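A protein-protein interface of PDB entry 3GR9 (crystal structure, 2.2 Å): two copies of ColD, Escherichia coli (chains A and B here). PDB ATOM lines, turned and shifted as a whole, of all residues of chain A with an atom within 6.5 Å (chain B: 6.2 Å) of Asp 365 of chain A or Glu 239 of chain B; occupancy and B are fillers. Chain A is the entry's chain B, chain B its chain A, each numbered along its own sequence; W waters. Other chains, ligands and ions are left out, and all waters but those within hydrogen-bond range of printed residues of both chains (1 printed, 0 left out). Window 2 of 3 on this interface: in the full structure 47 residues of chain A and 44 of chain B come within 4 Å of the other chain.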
ATOM      1  N   ILE A 309     -18.297 -34.265 -18.970  1.00  0.00           N
ATOM      2  CA  ILE A 309     -17.309 -33.474 -19.676  1.00  0.00           C
ATOM      3  C   ILE A 309     -16.224 -34.416 -20.295  1.00  0.00           C
ATOM      4  O   ILE A 309     -15.568 -35.170 -19.633  1.00  0.00           O
ATOM      5  CB  ILE A 309     -16.765 -32.385 -18.719  1.00  0.00           C
ATOM      6  CG1 ILE A 309     -16.824 -31.025 -19.412  1.00  0.00           C
ATOM      7  CG2 ILE A 309     -15.344 -32.705 -18.297  1.00  0.00           C
ATOM      8  CD1 ILE A 309     -18.065 -30.191 -19.100  1.00  0.00           C
ATOM      9  N   ARG A 318     -17.701 -35.717 -29.244  1.00  0.00           N
ATOM     10  CA  ARG A 318     -19.005 -35.384 -28.697  1.00  0.00           C
ATOM     11  C   ARG A 318     -20.226 -35.832 -29.498  1.00  0.00           C
ATOM     12  O   ARG A 318     -21.158 -36.462 -28.939  1.00  0.00           O
ATOM     13  CB  ARG A 318     -19.112 -33.910 -28.298  1.00  0.00           C
ATOM     14  CG  ARG A 318     -20.278 -33.621 -27.349  1.00  0.00           C
ATOM     15  CD  ARG A 318     -21.394 -32.869 -28.062  1.00  0.00           C
ATOM     16  NE  ARG A 318     -20.984 -31.562 -28.590  1.00  0.00           N
ATOM     17  CZ  ARG A 318     -20.825 -30.480 -27.825  1.00  0.00           C
ATOM     18  NH1 ARG A 318     -20.976 -30.560 -26.506  1.00  0.00           N
ATOM     19  NH2 ARG A 318     -20.483 -29.315 -28.350  1.00  0.00           N
ATOM     20  N   PRO A 334     -27.026 -29.749 -24.476  1.00  0.00           N
ATOM     21  CA  PRO A 334     -25.921 -28.901 -24.063  1.00  0.00           C
ATOM     22  C   PRO A 334     -26.079 -28.573 -22.590  1.00  0.00           C
ATOM     23  O   PRO A 334     -27.195 -28.406 -22.113  1.00  0.00           O
ATOM     24  CB  PRO A 334     -26.173 -27.598 -24.859  1.00  0.00           C
ATOM     25  CG  PRO A 334     -26.786 -28.053 -26.095  1.00  0.00           C
ATOM     26  CD  PRO A 334     -27.685 -29.230 -25.686  1.00  0.00           C
ATOM     27  N   THR A 337     -26.559 -23.650 -21.645  1.00  0.00           N
ATOM     28  CA  THR A 337     -26.501 -23.199 -23.036  1.00  0.00           C
ATOM     29  C   THR A 337     -25.057 -23.218 -23.553  1.00  0.00           C
ATOM     30  O   THR A 337     -24.781 -22.732 -24.654  1.00  0.00           O
ATOM     31  CB  THR A 337     -27.121 -21.763 -23.207  1.00  0.00           C
ATOM     32  OG1 THR A 337     -26.193 -20.788 -22.715  1.00  0.00           O
ATOM     33  CG2 THR A 337     -28.466 -21.606 -22.437  1.00  0.00           C
ATOM     34  N   GLY A 338     -24.142 -23.812 -22.784  1.00  0.00           N
ATOM     35  CA  GLY A 338     -22.727 -23.912 -23.207  1.00  0.00           C
ATOM     36  C   GLY A 338     -22.033 -22.583 -22.975  1.00  0.00           C
ATOM     37  O   GLY A 338     -22.321 -21.864 -21.994  1.00  0.00           O
ATOM     38  N   ASN A 339     -21.154 -22.232 -23.907  1.00  0.00           N
ATOM     39  CA  ASN A 339     -20.404 -20.991 -23.803  1.00  0.00           C
ATOM     40  C   ASN A 339     -21.258 -19.811 -24.152  1.00  0.00           C
ATOM     41  O   ASN A 339     -21.394 -19.451 -25.324  1.00  0.00           O
ATOM     42  CB  ASN A 339     -19.210 -20.958 -24.749  1.00  0.00           C
ATOM     43  CG  ASN A 339     -18.316 -19.715 -24.509  1.00  0.00           C
ATOM     44  OD1 ASN A 339     -18.677 -18.759 -23.800  1.00  0.00           O
ATOM     45  ND2 ASN A 339     -17.157 -19.718 -25.128  1.00  0.00           N
ATOM     46  N   PHE A 340     -21.742 -19.119 -23.142  1.00  0.00           N
ATOM     47  CA  PHE A 340     -22.560 -17.984 -23.503  1.00  0.00           C
ATOM     48  C   PHE A 340     -21.896 -16.987 -24.457  1.00  0.00           C
ATOM     49  O   PHE A 340     -22.543 -16.252 -25.217  1.00  0.00           O
ATOM     50  CB  PHE A 340     -23.096 -17.263 -22.285  1.00  0.00           C
ATOM     51  CG  PHE A 340     -24.012 -16.161 -22.663  1.00  0.00           C
ATOM     52  CD1 PHE A 340     -25.318 -16.470 -23.039  1.00  0.00           C
ATOM     53  CD2 PHE A 340     -23.530 -14.886 -22.884  1.00  0.00           C
ATOM     54  CE1 PHE A 340     -26.188 -15.499 -23.499  1.00  0.00           C
ATOM     55  CE2 PHE A 340     -24.382 -13.884 -23.367  1.00  0.00           C
ATOM     56  CZ  PHE A 340     -25.724 -14.194 -23.658  1.00  0.00           C
ATOM     57  N   LYS A 342     -20.387 -17.408 -27.108  1.00  0.00           N
ATOM     58  CA  LYS A 342     -20.337 -17.734 -28.517  1.00  0.00           C
ATOM     59  C   LYS A 342     -21.471 -16.986 -29.185  1.00  0.00           C
ATOM     60  O   LYS A 342     -21.601 -16.992 -30.409  1.00  0.00           O
ATOM     61  CB  LYS A 342     -20.532 -19.247 -28.719  1.00  0.00           C
ATOM     62  CG  LYS A 342     -21.765 -19.915 -28.072  1.00  0.00           C
ATOM     63  CD  LYS A 342     -21.874 -21.381 -28.612  1.00  0.00           C
ATOM     64  CE  LYS A 342     -22.776 -22.239 -27.780  1.00  0.00           C
ATOM     65  NZ  LYS A 342     -23.618 -21.379 -26.910  1.00  0.00           N
ATOM     66  N   ASP A 359     -11.525 -20.188 -21.467  1.00  0.00           N
ATOM     67  CA  ASP A 359     -11.080 -21.460 -22.028  1.00  0.00           C
ATOM     68  C   ASP A 359     -11.909 -22.651 -21.492  1.00  0.00           C
ATOM     69  O   ASP A 359     -12.316 -23.548 -22.224  1.00  0.00           O
ATOM     70  CB  ASP A 359      -9.581 -21.612 -21.750  1.00  0.00           C
ATOM     71  CG  ASP A 359      -8.713 -20.634 -22.582  1.00  0.00           C
ATOM     72  OD1 ASP A 359      -9.257 -19.733 -23.268  1.00  0.00           O
ATOM     73  OD2 ASP A 359      -7.464 -20.781 -22.573  1.00  0.00           O
ATOM     74  N   ASN A 360     -12.225 -22.603 -20.209  1.00  0.00           N
ATOM     75  CA  ASN A 360     -13.026 -23.657 -19.616  1.00  0.00           C
ATOM     76  C   ASN A 360     -14.394 -23.722 -20.254  1.00  0.00           C
ATOM     77  O   ASN A 360     -14.775 -24.785 -20.798  1.00  0.00           O
ATOM     78  CB  ASN A 360     -13.103 -23.494 -18.126  1.00  0.00           C
ATOM     79  CG  ASN A 360     -11.841 -23.939 -17.444  1.00  0.00           C
ATOM     80  OD1 ASN A 360     -11.055 -24.711 -17.997  1.00  0.00           O
ATOM     81  ND2 ASN A 360     -11.671 -23.489 -16.197  1.00  0.00           N
ATOM     82  N   ALA A 361     -15.074 -22.577 -20.299  1.00  0.00           N
ATOM     83  CA  ALA A 361     -16.380 -22.520 -20.933  1.00  0.00           C
ATOM     84  C   ALA A 361     -16.320 -22.884 -22.399  1.00  0.00           C
ATOM     85  O   ALA A 361     -17.237 -23.616 -22.874  1.00  0.00           O
ATOM     86  CB  ALA A 361     -16.998 -21.166 -20.688  1.00  0.00           C
ATOM     87  N   GLU A 362     -15.214 -22.476 -23.065  1.00  0.00           N
ATOM     88  CA  GLU A 362     -15.020 -22.832 -24.497  1.00  0.00           C
ATOM     89  C   GLU A 362     -14.951 -24.371 -24.588  1.00  0.00           C
ATOM     90  O   GLU A 362     -15.554 -25.023 -25.455  1.00  0.00           O
ATOM     91  CB  GLU A 362     -13.773 -22.170 -25.149  1.00  0.00           C
ATOM     92  CG  GLU A 362     -14.078 -20.859 -25.955  1.00  0.00           C
ATOM     93  CD  GLU A 362     -12.945 -19.802 -25.963  1.00  0.00           C
ATOM     94  OE1 GLU A 362     -11.755 -20.220 -25.973  1.00  0.00           O
ATOM     95  OE2 GLU A 362     -13.245 -18.571 -25.980  1.00  0.00           O
ATOM     96  N   TYR A 363     -14.291 -24.985 -23.618  1.00  0.00           N
ATOM     97  CA  TYR A 363     -14.092 -26.438 -23.557  1.00  0.00           C
ATOM     98  C   TYR A 363     -15.354 -27.165 -23.164  1.00  0.00           C
ATOM     99  O   TYR A 363     -15.751 -28.184 -23.742  1.00  0.00           O
ATOM    100  CB  TYR A 363     -12.923 -26.771 -22.639  1.00  0.00           C
ATOM    101  CG  TYR A 363     -12.643 -28.239 -22.712  1.00  0.00           C
ATOM    102  CD1 TYR A 363     -11.756 -28.763 -23.645  1.00  0.00           C
ATOM    103  CD2 TYR A 363     -13.384 -29.116 -21.939  1.00  0.00           C
ATOM    104  CE1 TYR A 363     -11.561 -30.104 -23.767  1.00  0.00           C
ATOM    105  CE2 TYR A 363     -13.217 -30.466 -22.064  1.00  0.00           C
ATOM    106  CZ  TYR A 363     -12.287 -30.952 -22.979  1.00  0.00           C
ATOM    107  OH  TYR A 363     -12.083 -32.307 -23.128  1.00  0.00           O
ATOM    108  N   LEU A 364     -16.054 -26.589 -22.201  1.00  0.00           N
ATOM    109  CA  LEU A 364     -17.352 -27.167 -21.873  1.00  0.00           C
ATOM    110  C   LEU A 364     -18.182 -26.976 -23.165  1.00  0.00           C
ATOM    111  O   LEU A 364     -18.992 -27.837 -23.490  1.00  0.00           O
ATOM    112  CB  LEU A 364     -18.018 -26.348 -20.746  1.00  0.00           C
ATOM    113  CG  LEU A 364     -19.511 -26.553 -20.457  1.00  0.00           C
ATOM    114  CD1 LEU A 364     -19.867 -26.101 -19.042  1.00  0.00           C
ATOM    115  CD2 LEU A 364     -20.485 -26.017 -21.526  1.00  0.00           C
ATOM    116  N   ASP A 365     -18.043 -25.850 -23.880  1.00  0.00           N
ATOM    117  CA  ASP A 365     -18.888 -25.694 -25.082  1.00  0.00           C
ATOM    118  C   ASP A 365     -18.773 -26.788 -26.126  1.00  0.00           C
ATOM    119  O   ASP A 365     -19.777 -27.137 -26.781  1.00  0.00           O
ATOM    120  CB  ASP A 365     -18.839 -24.308 -25.727  1.00  0.00           C
ATOM    121  CG  ASP A 365     -20.069 -24.037 -26.625  1.00  0.00           C
ATOM    122  OD1 ASP A 365     -21.086 -23.575 -26.053  1.00  0.00           O
ATOM    123  OD2 ASP A 365     -20.064 -24.259 -27.866  1.00  0.00           O
ATOM    124  N   LYS A 366     -17.576 -27.327 -26.309  1.00  0.00           N
ATOM    125  CA  LYS A 366     -17.378 -28.379 -27.289  1.00  0.00           C
ATOM    126  C   LYS A 366     -17.384 -29.804 -26.727  1.00  0.00           C
ATOM    127  O   LYS A 366     -17.544 -30.743 -27.477  1.00  0.00           O
ATOM    128  CB  LYS A 366     -16.109 -28.139 -28.109  1.00  0.00           C
ATOM    129  CG  LYS A 366     -15.813 -26.691 -28.429  1.00  0.00           C
ATOM    130  CD  LYS A 366     -15.948 -26.414 -29.908  1.00  0.00           C
ATOM    131  CE  LYS A 366     -15.238 -25.135 -30.309  1.00  0.00           C
ATOM    132  NZ  LYS A 366     -14.064 -25.384 -31.194  1.00  0.00           N
ATOM    133  N   ASN A 367     -17.208 -29.966 -25.421  1.00  0.00           N
ATOM    134  CA  ASN A 367     -17.098 -31.308 -24.832  1.00  0.00           C
ATOM    135  C   ASN A 367     -18.096 -31.723 -23.760  1.00  0.00           C
ATOM    136  O   ASN A 367     -17.967 -32.797 -23.173  1.00  0.00           O
ATOM    137  CB  ASN A 367     -15.688 -31.532 -24.308  1.00  0.00           C
ATOM    138  CG  ASN A 367     -14.650 -31.256 -25.351  1.00  0.00           C
ATOM    139  OD1 ASN A 367     -14.390 -32.087 -26.213  1.00  0.00           O
ATOM    140  ND2 ASN A 367     -14.064 -30.071 -25.296  1.00  0.00           N
ATOM    141  N   GLY A 368     -19.089 -30.886 -23.518  1.00  0.00           N
ATOM    142  CA  GLY A 368     -20.062 -31.173 -22.495  1.00  0.00           C
ATOM    143  C   GLY A 368     -21.448 -31.552 -22.950  1.00  0.00           C
ATOM    144  O   GLY A 368     -21.946 -31.042 -23.921  1.00  0.00           O
ATOM    145  N   SER B 234     -30.099 -23.589 -38.697  1.00  0.00           N
ATOM    146  CA  SER B 234     -29.399 -24.794 -39.044  1.00  0.00           C
ATOM    147  C   SER B 234     -30.224 -25.951 -38.537  1.00  0.00           C
ATOM    148  O   SER B 234     -31.195 -25.772 -37.786  1.00  0.00           O
ATOM    149  CB  SER B 234     -28.048 -24.824 -38.352  1.00  0.00           C
ATOM    150  OG  SER B 234     -27.825 -26.110 -37.802  1.00  0.00           O
ATOM    151  N   ASP B 236     -28.718 -28.651 -36.881  1.00  0.00           N
ATOM    152  CA  ASP B 236     -28.183 -29.185 -35.646  1.00  0.00           C
ATOM    153  C   ASP B 236     -28.807 -28.463 -34.455  1.00  0.00           C
ATOM    154  O   ASP B 236     -28.357 -27.373 -34.063  1.00  0.00           O
ATOM    155  CB  ASP B 236     -26.660 -29.051 -35.655  1.00  0.00           C
ATOM    156  CG  ASP B 236     -26.020 -29.720 -34.458  1.00  0.00           C
ATOM    157  OD1 ASP B 236     -26.688 -30.613 -33.868  1.00  0.00           O
ATOM    158  OD2 ASP B 236     -24.867 -29.350 -34.123  1.00  0.00           O
ATOM    159  N   GLN B 237     -29.867 -29.052 -33.911  1.00  0.00           N
ATOM    160  CA  GLN B 237     -30.568 -28.456 -32.766  1.00  0.00           C
ATOM    161  C   GLN B 237     -29.670 -28.416 -31.558  1.00  0.00           C
ATOM    162  O   GLN B 237     -29.797 -27.555 -30.663  1.00  0.00           O
ATOM    163  CB  GLN B 237     -31.779 -29.286 -32.379  1.00  0.00           C
ATOM    164  CG  GLN B 237     -32.441 -29.893 -33.589  1.00  0.00           C
ATOM    165  CD  GLN B 237     -33.788 -29.262 -33.807  1.00  0.00           C
ATOM    166  OE1 GLN B 237     -34.493 -28.989 -32.819  1.00  0.00           O
ATOM    167  NE2 GLN B 237     -34.201 -29.072 -35.082  1.00  0.00           N
ATOM    168  N   PHE B 238     -28.706 -29.329 -31.537  1.00  0.00           N
ATOM    169  CA  PHE B 238     -27.808 -29.309 -30.421  1.00  0.00           C
ATOM    170  C   PHE B 238     -27.407 -27.860 -30.253  1.00  0.00           C
ATOM    171  O   PHE B 238     -27.514 -27.305 -29.146  1.00  0.00           O
ATOM    172  CB  PHE B 238     -26.630 -30.258 -30.586  1.00  0.00           C
ATOM    173  CG  PHE B 238     -26.057 -30.699 -29.282  1.00  0.00           C
ATOM    174  CD1 PHE B 238     -26.613 -31.764 -28.597  1.00  0.00           C
ATOM    175  CD2 PHE B 238     -25.057 -29.959 -28.681  1.00  0.00           C
ATOM    176  CE1 PHE B 238     -26.109 -32.146 -27.355  1.00  0.00           C
ATOM    177  CE2 PHE B 238     -24.532 -30.335 -27.461  1.00  0.00           C
ATOM    178  CZ  PHE B 238     -25.072 -31.425 -26.785  1.00  0.00           C
ATOM    179  N   GLU B 239     -27.062 -27.251 -31.394  1.00  0.00           N
ATOM    180  CA  GLU B 239     -26.665 -25.864 -31.473  1.00  0.00           C
ATOM    181  C   GLU B 239     -27.864 -24.919 -31.660  1.00  0.00           C
ATOM    182  O   GLU B 239     -28.237 -24.230 -30.719  1.00  0.00           O
ATOM    183  CB  GLU B 239     -25.585 -25.675 -32.548  1.00  0.00           C
ATOM    184  CG  GLU B 239     -24.331 -24.892 -32.057  1.00  0.00           C
ATOM    185  CD  GLU B 239     -23.124 -25.778 -31.651  1.00  0.00           C
ATOM    186  OE1 GLU B 239     -23.009 -26.917 -32.170  1.00  0.00           O
ATOM    187  OE2 GLU B 239     -22.280 -25.325 -30.827  1.00  0.00           O
ATOM    188  N   GLU B 240     -28.492 -24.909 -32.835  1.00  0.00           N
ATOM    189  CA  GLU B 240     -29.612 -23.986 -33.078  1.00  0.00           C
ATOM    190  C   GLU B 240     -30.523 -23.722 -31.856  1.00  0.00           C
ATOM    191  O   GLU B 240     -30.833 -22.586 -31.492  1.00  0.00           O
ATOM    192  CB  GLU B 240     -30.469 -24.475 -34.262  1.00  0.00           C
ATOM    193  CG  GLU B 240     -31.382 -23.394 -34.927  1.00  0.00           C
ATOM    194  CD  GLU B 240     -30.723 -22.001 -35.078  1.00  0.00           C
ATOM    195  OE1 GLU B 240     -29.480 -21.918 -35.044  1.00  0.00           O
ATOM    196  OE2 GLU B 240     -31.447 -21.008 -35.356  1.00  0.00           O
ATOM    197  N   SER B 241     -31.022 -24.796 -31.285  1.00  0.00           N
ATOM    198  CA  SER B 241     -31.954 -24.719 -30.187  1.00  0.00           C
ATOM    199  C   SER B 241     -31.405 -24.027 -28.940  1.00  0.00           C
ATOM    200  O   SER B 241     -32.167 -23.738 -28.002  1.00  0.00           O
ATOM    201  CB  SER B 241     -32.469 -26.126 -29.870  1.00  0.00           C
ATOM    202  OG  SER B 241     -33.796 -26.296 -30.327  1.00  0.00           O
ATOM    203  N   PHE B 242     -30.105 -23.728 -28.949  1.00  0.00           N
ATOM    204  CA  PHE B 242     -29.473 -22.994 -27.837  1.00  0.00           C
ATOM    205  C   PHE B 242     -28.704 -21.699 -28.201  1.00  0.00           C
ATOM    206  O   PHE B 242     -27.828 -21.214 -27.486  1.00  0.00           O
ATOM    207  CB  PHE B 242     -28.659 -23.972 -27.025  1.00  0.00           C
ATOM    208  CG  PHE B 242     -29.479 -25.079 -26.481  1.00  0.00           C
ATOM    209  CD1 PHE B 242     -30.097 -24.914 -25.250  1.00  0.00           C
ATOM    210  CD2 PHE B 242     -29.736 -26.224 -27.235  1.00  0.00           C
ATOM    211  CE1 PHE B 242     -30.856 -25.946 -24.694  1.00  0.00           C
ATOM    212  CE2 PHE B 242     -30.505 -27.237 -26.701  1.00  0.00           C
ATOM    213  CZ  PHE B 242     -31.070 -27.101 -25.428  1.00  0.00           C
ATOM    214  N   LYS B 243     -29.105 -21.091 -29.307  1.00  0.00           N
ATOM    215  CA  LYS B 243     -28.484 -19.871 -29.782  1.00  0.00           C
ATOM    216  C   LYS B 243     -29.425 -18.736 -29.331  1.00  0.00           C
ATOM    217  O   LYS B 243     -30.609 -18.965 -29.098  1.00  0.00           O
ATOM    218  CB  LYS B 243     -28.263 -20.030 -31.307  1.00  0.00           C
ATOM    219  CG  LYS B 243     -28.183 -18.779 -32.164  1.00  0.00           C
ATOM    220  CD  LYS B 243     -27.338 -19.050 -33.406  1.00  0.00           C
ATOM    221  CE  LYS B 243     -27.811 -18.275 -34.636  1.00  0.00           C
ATOM    222  NZ  LYS B 243     -28.299 -19.164 -35.761  1.00  0.00           N
HETATM  223  O   HOH W   1     -25.629 -20.545 -25.678  1.00  0.00           O
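Among the printed residues, pairs that only touch across the chains: Arg 318 of chain A with Phe 238 of chain B, Pro 334 of chain A with Phe 238 of chain B, Pro 334 of chain A with Phe 242 of chain B and Asp 365 of chain A with Glu 239 of chain B.
Printed residues of chain A that touch a printed residue of chain B: Arg 318, Pro 334 and Asp 365. Of the 9 printed residues of chain B, 3 touch a printed residue of chain A. Hydrophobic or aromatic side chains of chain B that line the printed part of chain A: Phe 238 and Phe 242. Among the printed residues, 4 pairs touch across the chains. Among the printed residues, no Asp or Glu carboxylate lies within 4 Å of a Lys or Arg side-chain nitrogen of the other chain.
Water W1 lies within hydrogen-bond range of NZ of Lys 342 of chain A (2.5 Å), O of Thr 337 of chain A (2.6 Å) and O of Phe 242 of chain B (2.9 Å).
OD1 of Asp 236 of chain B lies close to N of Phe 238 of chain B (3.3 Å). The backbone carbonyl oxygen (O) of Asp 365 of chain A lies within hydrogen-bond range of the guanidinium group (NH2) of Arg 318 of chain A (2.8 Å). The backbone carbonyl oxygen (O) of Lys 366 of chain A sits close to the guanidinium group (NH2) of Arg 318 of chain A (3.4 Å). NH1 of Arg 318 of chain A sits at hydrogen-bond distance from O of Gly 368 of chain A, 2.8 Å away. N of Asn 339 of chain A lies within hydrogen-bond range of OD1 of Asp 365 of chain A. The side-chain amino group of Lys 342 of chain A lies within salt-bridge range of the side-chain carboxylate of Asp 365 of chain A (3.5 Å).
Printed residues of chain B within 4 Å of Arg 318 of chain A: Phe 238. Printed residues of chain B within 4 Å of Pro 334 of chain A: Phe 238 and Phe 242. Asp 365 of chain A touches just one residue of chain B: Glu 239. Gly 368 of chain A touches none of the printed residues of chain B. Of the printed residues of chain A, Phe 238 of chain B touches Arg 318 and Pro 334. The nearest residue of chain A that does not touch Glu 239 of chain B is Lys 342 of chain A (4.4 Å).
No position is printed for both chains.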
